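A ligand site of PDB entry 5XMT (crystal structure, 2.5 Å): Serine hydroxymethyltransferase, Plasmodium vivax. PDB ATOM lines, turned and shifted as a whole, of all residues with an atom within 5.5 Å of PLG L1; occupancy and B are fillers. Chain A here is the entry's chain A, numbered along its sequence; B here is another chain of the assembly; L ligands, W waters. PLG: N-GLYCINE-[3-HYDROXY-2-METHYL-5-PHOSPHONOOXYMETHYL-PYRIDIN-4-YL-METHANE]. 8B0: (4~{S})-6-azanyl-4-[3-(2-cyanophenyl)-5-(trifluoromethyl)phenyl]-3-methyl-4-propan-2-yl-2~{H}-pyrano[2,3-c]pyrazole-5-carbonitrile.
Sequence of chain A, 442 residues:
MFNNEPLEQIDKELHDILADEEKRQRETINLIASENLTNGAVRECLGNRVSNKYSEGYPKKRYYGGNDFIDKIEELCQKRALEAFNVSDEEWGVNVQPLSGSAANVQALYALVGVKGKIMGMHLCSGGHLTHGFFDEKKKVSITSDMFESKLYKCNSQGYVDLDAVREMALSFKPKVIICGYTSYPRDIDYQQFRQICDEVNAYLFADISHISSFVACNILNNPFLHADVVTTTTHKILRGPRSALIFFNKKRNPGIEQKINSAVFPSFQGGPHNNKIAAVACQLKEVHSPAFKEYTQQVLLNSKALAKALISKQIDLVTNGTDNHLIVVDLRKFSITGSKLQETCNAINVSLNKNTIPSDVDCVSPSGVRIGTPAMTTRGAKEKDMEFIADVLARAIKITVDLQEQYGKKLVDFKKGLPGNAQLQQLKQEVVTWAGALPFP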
ATOM      1  N   ILE A  32     -25.902 -31.571  14.028  1.00  0.00           N
ATOM      2  CA  ILE A  32     -25.929 -30.455  13.083  1.00  0.00           C
ATOM      3  C   ILE A  32     -27.280 -29.792  13.254  1.00  0.00           C
ATOM      4  O   ILE A  32     -28.297 -30.429  13.062  1.00  0.00           O
ATOM      5  CB  ILE A  32     -25.743 -30.877  11.600  1.00  0.00           C
ATOM      6  CG1 ILE A  32     -24.447 -31.676  11.393  1.00  0.00           C
ATOM      7  CG2 ILE A  32     -25.743 -29.650  10.699  1.00  0.00           C
ATOM      8  CD1 ILE A  32     -23.196 -30.831  11.397  1.00  0.00           C
ATOM      9  N   SER A  34     -28.947 -27.671  11.666  1.00  0.00           N
ATOM     10  CA  SER A  34     -29.725 -27.563  10.456  1.00  0.00           C
ATOM     11  C   SER A  34     -30.156 -28.885   9.797  1.00  0.00           C
ATOM     12  O   SER A  34     -30.809 -28.842   8.767  1.00  0.00           O
ATOM     13  CB  SER A  34     -28.932 -26.746   9.434  1.00  0.00           C
ATOM     14  OG  SER A  34     -27.599 -27.199   9.364  1.00  0.00           O
ATOM     15  N   SER A 100     -34.699 -23.792  -2.963  1.00  0.00           N
ATOM     16  CA  SER A 100     -34.018 -23.894  -1.653  1.00  0.00           C
ATOM     17  C   SER A 100     -34.059 -22.574  -0.894  1.00  0.00           C
ATOM     18  O   SER A 100     -34.588 -21.570  -1.367  1.00  0.00           O
ATOM     19  CB  SER A 100     -32.547 -24.355  -1.835  1.00  0.00           C
ATOM     20  OG  SER A 100     -32.175 -25.379  -0.910  1.00  0.00           O
ATOM     21  N   GLY A 101     -33.507 -22.583   0.297  1.00  0.00           N
ATOM     22  CA  GLY A 101     -33.532 -21.396   1.147  1.00  0.00           C
ATOM     23  C   GLY A 101     -32.887 -20.194   0.518  1.00  0.00           C
ATOM     24  O   GLY A 101     -33.425 -19.095   0.581  1.00  0.00           O
ATOM     25  N   SER A 102     -31.735 -20.425  -0.106  1.00  0.00           N
ATOM     26  CA  SER A 102     -30.922 -19.342  -0.657  1.00  0.00           C
ATOM     27  C   SER A 102     -31.588 -18.742  -1.889  1.00  0.00           C
ATOM     28  O   SER A 102     -31.607 -17.551  -2.072  1.00  0.00           O
ATOM     29  CB  SER A 102     -29.491 -19.816  -0.982  1.00  0.00           C
ATOM     30  OG  SER A 102     -28.782 -20.208   0.199  1.00  0.00           O
ATOM     31  N   ALA A 103     -32.131 -19.582  -2.747  1.00  0.00           N
ATOM     32  CA  ALA A 103     -32.911 -19.074  -3.867  1.00  0.00           C
ATOM     33  C   ALA A 103     -34.097 -18.205  -3.405  1.00  0.00           C
ATOM     34  O   ALA A 103     -34.299 -17.119  -3.935  1.00  0.00           O
ATOM     35  CB  ALA A 103     -33.389 -20.216  -4.737  1.00  0.00           C
ATOM     36  N   ASN A 105     -34.540 -16.576  -0.447  1.00  0.00           N
ATOM     37  CA  ASN A 105     -34.098 -15.262   0.065  1.00  0.00           C
ATOM     38  C   ASN A 105     -33.721 -14.284  -1.064  1.00  0.00           C
ATOM     39  O   ASN A 105     -34.110 -13.120  -1.007  1.00  0.00           O
ATOM     40  CB  ASN A 105     -32.924 -15.386   1.030  1.00  0.00           C
ATOM     41  CG  ASN A 105     -33.316 -15.929   2.385  1.00  0.00           C
ATOM     42  OD1 ASN A 105     -34.460 -16.328   2.614  1.00  0.00           O
ATOM     43  ND2 ASN A 105     -32.363 -15.944   3.298  1.00  0.00           N
ATOM     44  N   HIS A 129     -27.149 -15.546   7.865  1.00  0.00           N
ATOM     45  CA  HIS A 129     -26.889 -16.339   6.686  1.00  0.00           C
ATOM     46  C   HIS A 129     -26.144 -15.546   5.627  1.00  0.00           C
ATOM     47  O   HIS A 129     -26.140 -14.322   5.632  1.00  0.00           O
ATOM     48  CB  HIS A 129     -28.188 -16.910   6.118  1.00  0.00           C
ATOM     49  CG  HIS A 129     -27.958 -18.100   5.243  1.00  0.00           C
ATOM     50  ND1 HIS A 129     -28.142 -18.049   3.883  1.00  0.00           N
ATOM     51  CD2 HIS A 129     -27.467 -19.320   5.516  1.00  0.00           C
ATOM     52  CE1 HIS A 129     -27.809 -19.215   3.352  1.00  0.00           C
ATOM     53  NE2 HIS A 129     -27.403 -20.002   4.319  1.00  0.00           N
ATOM     54  N   THR A 131     -27.008 -15.341   2.547  1.00  0.00           N
ATOM     55  CA  THR A 131     -28.052 -14.611   1.783  1.00  0.00           C
ATOM     56  C   THR A 131     -28.644 -13.367   2.505  1.00  0.00           C
ATOM     57  O   THR A 131     -29.590 -12.765   1.996  1.00  0.00           O
ATOM     58  CB  THR A 131     -29.207 -15.540   1.395  1.00  0.00           C
ATOM     59  OG1 THR A 131     -29.793 -16.092   2.576  1.00  0.00           O
ATOM     60  CG2 THR A 131     -28.706 -16.648   0.499  1.00  0.00           C
ATOM     61  N   HIS A 132     -28.106 -12.995   3.666  1.00  0.00           N
ATOM     62  CA  HIS A 132     -28.493 -11.768   4.363  1.00  0.00           C
ATOM     63  C   HIS A 132     -27.556 -10.615   4.063  1.00  0.00           C
ATOM     64  O   HIS A 132     -27.489  -9.655   4.814  1.00  0.00           O
ATOM     65  CB  HIS A 132     -28.639 -11.999   5.872  1.00  0.00           C
ATOM     66  CG  HIS A 132     -29.638 -13.066   6.224  1.00  0.00           C
ATOM     67  ND1 HIS A 132     -29.777 -13.562   7.494  1.00  0.00           N
ATOM     68  CD2 HIS A 132     -30.508 -13.765   5.455  1.00  0.00           C
ATOM     69  CE1 HIS A 132     -30.714 -14.495   7.504  1.00  0.00           C
ATOM     70  NE2 HIS A 132     -31.170 -14.635   6.268  1.00  0.00           N
ATOM     71  N   GLY A 181     -33.913 -13.121  11.856  1.00  0.00           N
ATOM     72  CA  GLY A 181     -33.953 -14.588  11.747  1.00  0.00           C
ATOM     73  C   GLY A 181     -32.628 -15.108  11.205  1.00  0.00           C
ATOM     74  O   GLY A 181     -32.088 -14.575  10.237  1.00  0.00           O
ATOM     75  N   TYR A 182     -32.079 -16.146  11.842  1.00  0.00           N
ATOM     76  CA  TYR A 182     -30.659 -16.430  11.701  1.00  0.00           C
ATOM     77  C   TYR A 182     -30.272 -17.903  11.547  1.00  0.00           C
ATOM     78  O   TYR A 182     -31.108 -18.778  11.669  1.00  0.00           O
ATOM     79  CB  TYR A 182     -29.927 -15.808  12.870  1.00  0.00           C
ATOM     80  CG  TYR A 182     -30.355 -14.379  13.154  1.00  0.00           C
ATOM     81  CD1 TYR A 182     -29.919 -13.321  12.356  1.00  0.00           C
ATOM     82  CD2 TYR A 182     -31.183 -14.081  14.223  1.00  0.00           C
ATOM     83  CE1 TYR A 182     -30.286 -12.023  12.625  1.00  0.00           C
ATOM     84  CE2 TYR A 182     -31.554 -12.775  14.503  1.00  0.00           C
ATOM     85  CZ  TYR A 182     -31.092 -11.747  13.700  1.00  0.00           C
ATOM     86  OH  TYR A 182     -31.453 -10.438  13.935  1.00  0.00           O
ATOM     87  N   THR A 183     -28.993 -18.140  11.254  1.00  0.00           N
ATOM     88  CA  THR A 183     -28.507 -19.488  11.029  1.00  0.00           C
ATOM     89  C   THR A 183     -27.937 -20.095  12.289  1.00  0.00           C
ATOM     90  O   THR A 183     -28.087 -21.292  12.499  1.00  0.00           O
ATOM     91  CB  THR A 183     -27.549 -19.676   9.821  1.00  0.00           C
ATOM     92  OG1 THR A 183     -26.351 -20.362  10.225  1.00  0.00           O
ATOM     93  CG2 THR A 183     -27.198 -18.409   9.174  1.00  0.00           C
ATOM     94  N   ASP A 208     -36.284 -14.465   8.395  1.00  0.00           N
ATOM     95  CA  ASP A 208     -35.848 -15.800   7.985  1.00  0.00           C
ATOM     96  C   ASP A 208     -35.894 -16.763   9.166  1.00  0.00           C
ATOM     97  O   ASP A 208     -34.994 -16.757   9.988  1.00  0.00           O
ATOM     98  CB  ASP A 208     -34.426 -15.745   7.397  1.00  0.00           C
ATOM     99  CG  ASP A 208     -34.033 -17.049   6.715  1.00  0.00           C
ATOM    100  OD1 ASP A 208     -34.689 -18.101   6.918  1.00  0.00           O
ATOM    101  OD2 ASP A 208     -33.047 -17.002   5.958  1.00  0.00           O
ATOM    102  N   SER A 210     -36.036 -20.307   9.081  1.00  0.00           N
ATOM    103  CA  SER A 210     -35.644 -21.683   8.677  1.00  0.00           C
ATOM    104  C   SER A 210     -35.163 -22.601   9.791  1.00  0.00           C
ATOM    105  O   SER A 210     -35.490 -23.794   9.832  1.00  0.00           O
ATOM    106  CB  SER A 210     -34.502 -21.581   7.673  1.00  0.00           C
ATOM    107  OG  SER A 210     -34.765 -20.577   6.720  1.00  0.00           O
ATOM    108  N   HIS A 211     -34.349 -22.037  10.682  1.00  0.00           N
ATOM    109  CA  HIS A 211     -33.841 -22.789  11.826  1.00  0.00           C
ATOM    110  C   HIS A 211     -34.916 -23.043  12.897  1.00  0.00           C
ATOM    111  O   HIS A 211     -34.914 -24.086  13.572  1.00  0.00           O
ATOM    112  CB  HIS A 211     -32.585 -22.113  12.427  1.00  0.00           C
ATOM    113  CG  HIS A 211     -31.313 -22.694  11.895  1.00  0.00           C
ATOM    114  ND1 HIS A 211     -30.740 -23.838  12.399  1.00  0.00           N
ATOM    115  CD2 HIS A 211     -30.543 -22.335  10.837  1.00  0.00           C
ATOM    116  CE1 HIS A 211     -29.662 -24.136  11.709  1.00  0.00           C
ATOM    117  NE2 HIS A 211     -29.508 -23.224  10.773  1.00  0.00           N
ATOM    118  N   THR A 234     -36.836 -22.533   5.094  1.00  0.00           N
ATOM    119  CA  THR A 234     -36.558 -23.786   4.461  1.00  0.00           C
ATOM    120  C   THR A 234     -37.519 -24.808   4.996  1.00  0.00           C
ATOM    121  O   THR A 234     -38.081 -24.639   6.075  1.00  0.00           O
ATOM    122  CB  THR A 234     -35.098 -24.218   4.718  1.00  0.00           C
ATOM    123  OG1 THR A 234     -34.848 -24.286   6.134  1.00  0.00           O
ATOM    124  CG2 THR A 234     -34.132 -23.260   4.031  1.00  0.00           C
ATOM    125  N   HIS A 236     -36.377 -28.099   5.198  1.00  0.00           N
ATOM    126  CA  HIS A 236     -35.538 -29.296   5.477  1.00  0.00           C
ATOM    127  C   HIS A 236     -34.929 -29.380   6.867  1.00  0.00           C
ATOM    128  O   HIS A 236     -34.411 -30.443   7.233  1.00  0.00           O
ATOM    129  CB  HIS A 236     -34.429 -29.524   4.428  1.00  0.00           C
ATOM    130  CG  HIS A 236     -33.683 -28.296   4.028  1.00  0.00           C
ATOM    131  ND1 HIS A 236     -34.198 -27.390   3.143  1.00  0.00           N
ATOM    132  CD2 HIS A 236     -32.443 -27.846   4.352  1.00  0.00           C
ATOM    133  CE1 HIS A 236     -33.323 -26.426   2.929  1.00  0.00           C
ATOM    134  NE2 HIS A 236     -32.239 -26.685   3.651  1.00  0.00           N
ATOM    135  N   LYS A 237     -35.000 -28.319   7.657  1.00  0.00           N
ATOM    136  CA  LYS A 237     -34.359 -28.358   8.941  1.00  0.00           C
ATOM    137  C   LYS A 237     -35.343 -28.880  10.000  1.00  0.00           C
ATOM    138  O   LYS A 237     -35.783 -30.041   9.892  1.00  0.00           O
ATOM    139  CB  LYS A 237     -33.776 -26.987   9.283  1.00  0.00           C
ATOM    140  CG  LYS A 237     -32.925 -26.377   8.200  1.00  0.00           C
ATOM    141  CD  LYS A 237     -32.393 -25.065   8.718  1.00  0.00           C
ATOM    142  CE  LYS A 237     -31.287 -24.497   7.880  1.00  0.00           C
ATOM    143  NZ  LYS A 237     -31.864 -23.817   6.710  1.00  0.00           N
ATOM    144  N   ARG A 243     -35.820 -30.805   0.938  1.00  0.00           N
ATOM    145  CA  ARG A 243     -35.029 -29.600   0.684  1.00  0.00           C
ATOM    146  C   ARG A 243     -35.783 -28.679  -0.271  1.00  0.00           C
ATOM    147  O   ARG A 243     -35.857 -28.921  -1.458  1.00  0.00           O
ATOM    148  CB  ARG A 243     -33.635 -29.901   0.156  1.00  0.00           C
ATOM    149  CG  ARG A 243     -32.890 -30.895   1.016  1.00  0.00           C
ATOM    150  CD  ARG A 243     -31.426 -31.012   0.567  1.00  0.00           C
ATOM    151  NE  ARG A 243     -30.666 -29.928   1.166  1.00  0.00           N
ATOM    152  CZ  ARG A 243     -30.102 -29.967   2.356  1.00  0.00           C
ATOM    153  NH1 ARG A 243     -30.159 -31.062   3.125  1.00  0.00           N
ATOM    154  NH2 ARG A 243     -29.457 -28.903   2.781  1.00  0.00           N
ATOM    155  N   SER A 244     -36.348 -27.615   0.293  1.00  0.00           N
ATOM    156  CA  SER A 244     -37.126 -26.643  -0.441  1.00  0.00           C
ATOM    157  C   SER A 244     -37.259 -25.440   0.468  1.00  0.00           C
ATOM    158  O   SER A 244     -36.718 -25.434   1.588  1.00  0.00           O
ATOM    159  CB  SER A 244     -38.505 -27.229  -0.756  1.00  0.00           C
ATOM    160  OG  SER A 244     -39.206 -26.489  -1.720  1.00  0.00           O
ATOM    161  N   ARG A 371     -21.267 -25.376  17.035  1.00  0.00           N
ATOM    162  CA  ARG A 371     -22.687 -25.269  17.108  1.00  0.00           C
ATOM    163  C   ARG A 371     -23.301 -26.654  17.110  1.00  0.00           C
ATOM    164  O   ARG A 371     -22.926 -27.500  16.309  1.00  0.00           O
ATOM    165  CB  ARG A 371     -23.227 -24.485  15.918  1.00  0.00           C
ATOM    166  CG  ARG A 371     -24.739 -24.311  15.907  1.00  0.00           C
ATOM    167  CD  ARG A 371     -25.193 -23.681  14.634  1.00  0.00           C
ATOM    168  NE  ARG A 371     -25.009 -24.574  13.495  1.00  0.00           N
ATOM    169  CZ  ARG A 371     -25.619 -24.456  12.310  1.00  0.00           C
ATOM    170  NH1 ARG A 371     -26.494 -23.487  12.083  1.00  0.00           N
ATOM    171  NH2 ARG A 371     -25.361 -25.340  11.358  1.00  0.00           N
ATOM    172  N   TYR B  54     -26.083 -32.076   4.841  1.00  0.00           N
ATOM    173  CA  TYR B  54     -25.623 -30.729   4.469  1.00  0.00           C
ATOM    174  C   TYR B  54     -24.168 -30.756   3.994  1.00  0.00           C
ATOM    175  O   TYR B  54     -23.306 -31.100   4.784  1.00  0.00           O
ATOM    176  CB  TYR B  54     -25.779 -29.734   5.633  1.00  0.00           C
ATOM    177  CG  TYR B  54     -26.744 -28.615   5.313  1.00  0.00           C
ATOM    178  CD1 TYR B  54     -26.438 -27.656   4.331  1.00  0.00           C
ATOM    179  CD2 TYR B  54     -27.981 -28.530   5.952  1.00  0.00           C
ATOM    180  CE1 TYR B  54     -27.329 -26.647   4.010  1.00  0.00           C
ATOM    181  CE2 TYR B  54     -28.874 -27.511   5.652  1.00  0.00           C
ATOM    182  CZ  TYR B  54     -28.552 -26.580   4.678  1.00  0.00           C
ATOM    183  OH  TYR B  54     -29.460 -25.584   4.353  1.00  0.00           O
ATOM    184  N   GLU B  56     -22.403 -28.095   2.049  1.00  0.00           N
ATOM    185  CA  GLU B  56     -21.931 -26.820   1.523  1.00  0.00           C
ATOM    186  C   GLU B  56     -20.453 -26.899   1.254  1.00  0.00           C
ATOM    187  O   GLU B  56     -19.681 -27.370   2.092  1.00  0.00           O
ATOM    188  CB  GLU B  56     -22.204 -25.716   2.533  1.00  0.00           C
ATOM    189  CG  GLU B  56     -23.667 -25.360   2.659  1.00  0.00           C
ATOM    190  CD  GLU B  56     -23.911 -24.413   3.810  1.00  0.00           C
ATOM    191  OE1 GLU B  56     -23.948 -24.881   4.966  1.00  0.00           O
ATOM    192  OE2 GLU B  56     -24.026 -23.185   3.535  1.00  0.00           O
ATOM    193  N   TYR B  64     -18.486 -28.791   6.583  1.00  0.00           N
ATOM    194  CA  TYR B  64     -18.737 -29.818   7.619  1.00  0.00           C
ATOM    195  C   TYR B  64     -18.026 -31.126   7.297  1.00  0.00           C
ATOM    196  O   TYR B  64     -17.763 -31.427   6.146  1.00  0.00           O
ATOM    197  CB  TYR B  64     -20.239 -30.133   7.783  1.00  0.00           C
ATOM    198  CG  TYR B  64     -21.185 -28.975   8.007  1.00  0.00           C
ATOM    199  CD1 TYR B  64     -20.732 -27.688   8.246  1.00  0.00           C
ATOM    200  CD2 TYR B  64     -22.563 -29.181   8.012  1.00  0.00           C
ATOM    201  CE1 TYR B  64     -21.589 -26.650   8.445  1.00  0.00           C
ATOM    202  CE2 TYR B  64     -23.454 -28.134   8.220  1.00  0.00           C
ATOM    203  CZ  TYR B  64     -22.949 -26.865   8.436  1.00  0.00           C
ATOM    204  OH  TYR B  64     -23.786 -25.798   8.648  1.00  0.00           O
ATOM    205  N   GLN B 270     -26.180 -20.353  -4.387  1.00  0.00           N
ATOM    206  CA  GLN B 270     -26.774 -21.437  -3.626  1.00  0.00           C
ATOM    207  C   GLN B 270     -26.160 -21.623  -2.249  1.00  0.00           C
ATOM    208  O   GLN B 270     -25.111 -21.082  -1.943  1.00  0.00           O
ATOM    209  CB  GLN B 270     -26.685 -22.740  -4.400  1.00  0.00           C
ATOM    210  CG  GLN B 270     -27.221 -22.617  -5.804  1.00  0.00           C
ATOM    211  CD  GLN B 270     -27.474 -23.940  -6.481  1.00  0.00           C
ATOM    212  OE1 GLN B 270     -28.316 -24.028  -7.395  1.00  0.00           O
ATOM    213  NE2 GLN B 270     -26.755 -24.983  -6.058  1.00  0.00           N
ATOM    214  N   GLY B 271     -26.874 -22.368  -1.411  1.00  0.00           N
ATOM    215  CA  GLY B 271     -26.362 -22.866  -0.145  1.00  0.00           C
ATOM    216  C   GLY B 271     -26.056 -24.352  -0.328  1.00  0.00           C
ATOM    217  O   GLY B 271     -25.298 -24.743  -1.203  1.00  0.00           O
ATOM    218  N   GLY B 272     -26.694 -25.188   0.486  1.00  0.00           N
ATOM    219  CA  GLY B 272     -26.414 -26.625   0.441  1.00  0.00           C
ATOM    220  C   GLY B 272     -26.783 -27.262  -0.900  1.00  0.00           C
ATOM    221  O   GLY B 272     -27.804 -26.928  -1.489  1.00  0.00           O
ATOM    222  N   HIS B 274     -28.156 -30.422  -3.166  1.00  0.00           N
ATOM    223  CA  HIS B 274     -29.188 -31.412  -2.979  1.00  0.00           C
ATOM    224  C   HIS B 274     -28.612 -32.709  -3.452  1.00  0.00           C
ATOM    225  O   HIS B 274     -28.543 -32.985  -4.645  1.00  0.00           O
ATOM    226  CB  HIS B 274     -30.430 -31.040  -3.771  1.00  0.00           C
ATOM    227  CG  HIS B 274     -31.150 -29.839  -3.239  1.00  0.00           C
ATOM    228  ND1 HIS B 274     -32.448 -29.572  -3.589  1.00  0.00           N
ATOM    229  CD2 HIS B 274     -30.767 -28.840  -2.413  1.00  0.00           C
ATOM    230  CE1 HIS B 274     -32.838 -28.449  -3.017  1.00  0.00           C
ATOM    231  NE2 HIS B 274     -31.834 -27.973  -2.297  1.00  0.00           N
HETATM  232  N1  PLG L   1     -31.704 -19.252   5.689  1.00  0.00           N
HETATM  233  C2  PLG L   1     -31.186 -19.652   6.872  1.00  0.00           C
HETATM  234  C2A PLG L   1     -31.544 -18.918   8.136  1.00  0.00           C
HETATM  235  C3  PLG L   1     -30.264 -20.791   6.904  1.00  0.00           C
HETATM  236  O3  PLG L   1     -29.714 -21.210   8.048  1.00  0.00           O
HETATM  237  C4  PLG L   1     -29.924 -21.460   5.639  1.00  0.00           C
HETATM  238  C4A PLG L   1     -28.958 -22.629   5.598  1.00  0.00           C
HETATM  239  C5  PLG L   1     -30.572 -20.939   4.408  1.00  0.00           C
HETATM  240  C6  PLG L   1     -31.436 -19.853   4.521  1.00  0.00           C
HETATM  241  C5A PLG L   1     -30.292 -21.525   3.038  1.00  0.00           C
HETATM  242  OP4 PLG L   1     -30.728 -22.857   2.850  1.00  0.00           O
HETATM  243  P   PLG L   1     -30.164 -23.664   1.577  1.00  0.00           P
HETATM  244  OP1 PLG L   1     -29.866 -22.694   0.481  1.00  0.00           O
HETATM  245  OP2 PLG L   1     -28.936 -24.335   2.138  1.00  0.00           O
HETATM  246  OP3 PLG L   1     -31.318 -24.604   1.356  1.00  0.00           O
HETATM  247  C   PLG L   1     -26.953 -24.319   8.221  1.00  0.00           C
HETATM  248  O   PLG L   1     -26.336 -25.385   8.383  1.00  0.00           O
HETATM  249  OXT PLG L   1     -27.511 -23.765   9.171  1.00  0.00           O
HETATM  250  CA  PLG L   1     -27.025 -23.685   6.841  1.00  0.00           C
HETATM  251  N   PLG L   1     -28.190 -22.828   6.819  1.00  0.00           N
HETATM  252  C2  8B0 L   2     -23.196 -19.029   9.156  1.00  0.00           C
HETATM  253  C3  8B0 L   2     -22.048 -19.711   9.429  1.00  0.00           C
HETATM  254  C4  8B0 L   2     -21.515 -20.834   8.546  1.00  0.00           C
HETATM  255  C5  8B0 L   2     -22.410 -21.033   7.354  1.00  0.00           C
HETATM  256  C6  8B0 L   2     -23.634 -20.274   7.107  1.00  0.00           C
HETATM  257  C10 8B0 L   2     -22.396 -21.933   6.159  1.00  0.00           C
HETATM  258  C12 8B0 L   2     -21.392 -22.983   5.743  1.00  0.00           C
HETATM  259  C13 8B0 L   2     -21.538 -22.119   9.426  1.00  0.00           C
HETATM  260  C14 8B0 L   2     -20.748 -23.305   8.853  1.00  0.00           C
HETATM  261  C15 8B0 L   2     -20.087 -20.497   8.077  1.00  0.00           C
HETATM  262  C16 8B0 L   2     -18.976 -20.696   8.911  1.00  0.00           C
HETATM  263  C17 8B0 L   2     -17.663 -20.433   8.522  1.00  0.00           C
HETATM  264  C19 8B0 L   2     -18.478 -19.717   6.394  1.00  0.00           C
HETATM  265  N53 8B0 L   2     -16.362 -16.719   6.415  1.00  0.00           N
HETATM  266  C50 8B0 L   2     -16.901 -17.353   5.631  1.00  0.00           C
HETATM  267  C39 8B0 L   2     -17.502 -18.051   4.746  1.00  0.00           C
HETATM  268  C40 8B0 L   2     -17.345 -17.602   3.443  1.00  0.00           C
HETATM  269  C41 8B0 L   2     -17.950 -18.280   2.401  1.00  0.00           C
HETATM  270  C42 8B0 L   2     -18.709 -19.420   2.681  1.00  0.00           C
HETATM  271  C43 8B0 L   2     -18.876 -19.877   3.977  1.00  0.00           C
HETATM  272  C32 8B0 L   2     -18.260 -19.191   5.026  1.00  0.00           C
HETATM  273  C18 8B0 L   2     -17.420 -19.926   7.253  1.00  0.00           C
HETATM  274  C33 8B0 L   2     -16.556 -20.664   9.537  1.00  0.00           C
HETATM  275  F48 8B0 L   2     -15.351 -20.711   8.987  1.00  0.00           F
HETATM  276  F47 8B0 L   2     -16.776 -21.783  10.228  1.00  0.00           F
HETATM  277  F46 8B0 L   2     -16.556 -19.624  10.351  1.00  0.00           F
HETATM  278  C20 8B0 L   2     -19.802 -19.993   6.797  1.00  0.00           C
HETATM  279  C34 8B0 L   2     -22.941 -22.565   9.877  1.00  0.00           C
HETATM  280  C8  8B0 L   2     -21.361 -19.456  10.465  1.00  0.00           C
HETATM  281  N9  8B0 L   2     -20.714 -19.237  11.411  1.00  0.00           N
HETATM  282  N7  8B0 L   2     -23.692 -18.055   9.917  1.00  0.00           N
HETATM  283  N51 8B0 L   2     -23.498 -21.609   5.437  1.00  0.00           N
HETATM  284  N11 8B0 L   2     -24.300 -20.589   5.976  1.00  0.00           N
HETATM  285  O1  8B0 L   2     -24.006 -19.320   8.001  1.00  0.00           O
HETATM  286  O   HOH W   1     -29.020 -24.156  -1.792  1.00  0.00           O
HETATM  287  O   HOH W   2     -29.953 -27.223   0.739  1.00  0.00           O
HETATM  288  O   HOH W   3     -26.778 -22.749   3.283  1.00  0.00           O
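OP3 of PLG L1 lies close to NE2 of His 236.
An oxygen (OP2) of PLG L1 lies within hydrogen-bond range of the side-chain hydroxyl (OH) of Tyr 54 of chain B, 2.6 Å away.
The side-chain hydroxyl (OG) of Ser 210 lies within hydrogen-bond range of a nitrogen (N1) of PLG L1 (3.5 Å).
The side-chain hydroxyl (OG) of Ser 100 lies within hydrogen-bond range of an oxygen (OP3) of PLG L1, at 2.5 Å.
NE2 of His 211 sits at hydrogen-bond distance from OXT of PLG L1 (2.6 Å).
The side-chain hydroxyl (OH) of Tyr 64 of chain B lies within hydrogen-bond range of an oxygen (O) of PLG L1, 2.6 Å away.
N of Gly 101 is in hydrogen-bond range of OP3 of PLG L1, 3.2 Å away.
OG of Ser 34 sits at hydrogen-bond distance from O of PLG L1 (2.4 Å).
OXT of PLG L1 lies within salt-bridge range of NH1 of Arg 371.
The side-chain hydroxyl of Ser 102 lies within hydrogen-bond range of an oxygen (OP1) of PLG L1.
The side-chain carboxylate (OE2) of Glu 56 of chain B is in hydrogen-bond range of a nitrogen (N51) of 8B0 L2.
OP2 of PLG L1 lies within hydrogen-bond range of N of Gly 272 of chain B (2.9 Å).
The backbone NH of Ser 102 is in hydrogen-bond range of an oxygen (OP1) of PLG L1 (3.0 Å).
OG1 of Thr 183 lies within hydrogen-bond range of O1 of 8B0 L2, 3.4 Å away.
OD2 of Asp 208 sits at hydrogen-bond distance from N1 of PLG L1, 2.6 Å away.
The side-chain hydroxyl (OH) of Tyr 54 of chain B is in hydrogen-bond range of a ring nitrogen (NE2) of His 236.
The side-chain carboxylate (OD2) of Asp 208 sits at hydrogen-bond distance from the side-chain amide nitrogen (ND2) of Asn 105, at 2.9 Å.
NE2 of His 132 is in hydrogen-bond range of OD2 of Asp 208 (3.0 Å).
A ring nitrogen (NE2) of His 211 lies close to the guanidinium group (NH1) of Arg 371.
The guanidinium group (NH2) of Arg 371 is in hydrogen-bond range of the side-chain hydroxyl (OH) of Tyr 64 of chain B, 3.2 Å away.
N of His 129 is in hydrogen-bond range of ND1 of His 132 (3.3 Å).
NH1 of Arg 371 lies within hydrogen-bond range of O of Thr 183.
The side-chain hydroxyl (OG) of Ser 100 is in hydrogen-bond range of a ring nitrogen (NE2) of His 274 of chain B (3.0 Å).
NE2 of His 129 touches C4 of PLG L1, 3.2 Å away.
Tyr 182 touches PLG L1.
CB of Thr 183 touches O3 of PLG L1 (3.2 Å).
Thr 234 touches PLG L1 (CG2 to OP4, 3.6 Å).
Lys 237 touches PLG L1.
OE1 of Glu 56 of chain B touches CA of PLG L1, at 3.8 Å.
N of Gly 271 of chain B touches OP1 of PLG L1 (3.6 Å).
Within 4 Å of PLG L1: Ser 34, Ser 100, Gly 101, Ser 102, His 129, Tyr 182, Thr 183, Asp 208, Ser 210, His 211, Thr 234, His 236, Lys 237, Arg 371, Tyr 54 of chain B, Glu 56 of chain B, Tyr 64 of chain B, Gly 271 of chain B and Gly 272 of chain B.
The nearest printed residue that does not touch PLG L1 is Asn 105 (4.1 Å).
Water W1 lies within hydrogen-bond range of the backbone NH (N) of Gly 271 of chain B (2.8 Å), an oxygen (OP1) of PLG L1 (2.8 Å), the backbone carbonyl oxygen (O) of Gly 272 of chain B (3.0 Å) and the side-chain hydroxyl (OG) of Ser 100 (3.5 Å).
Water W3 lies within hydrogen-bond range of OE2 of Glu 56 of chain B (2.8 Å), OP2 of PLG L1 (2.9 Å) and NE2 of His 129 (3.0 Å).
Water W2 lies within hydrogen-bond range of NH2 of Arg 243, OP3 of PLG L1, O of Gly 272 of chain B and OG of Ser 100.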
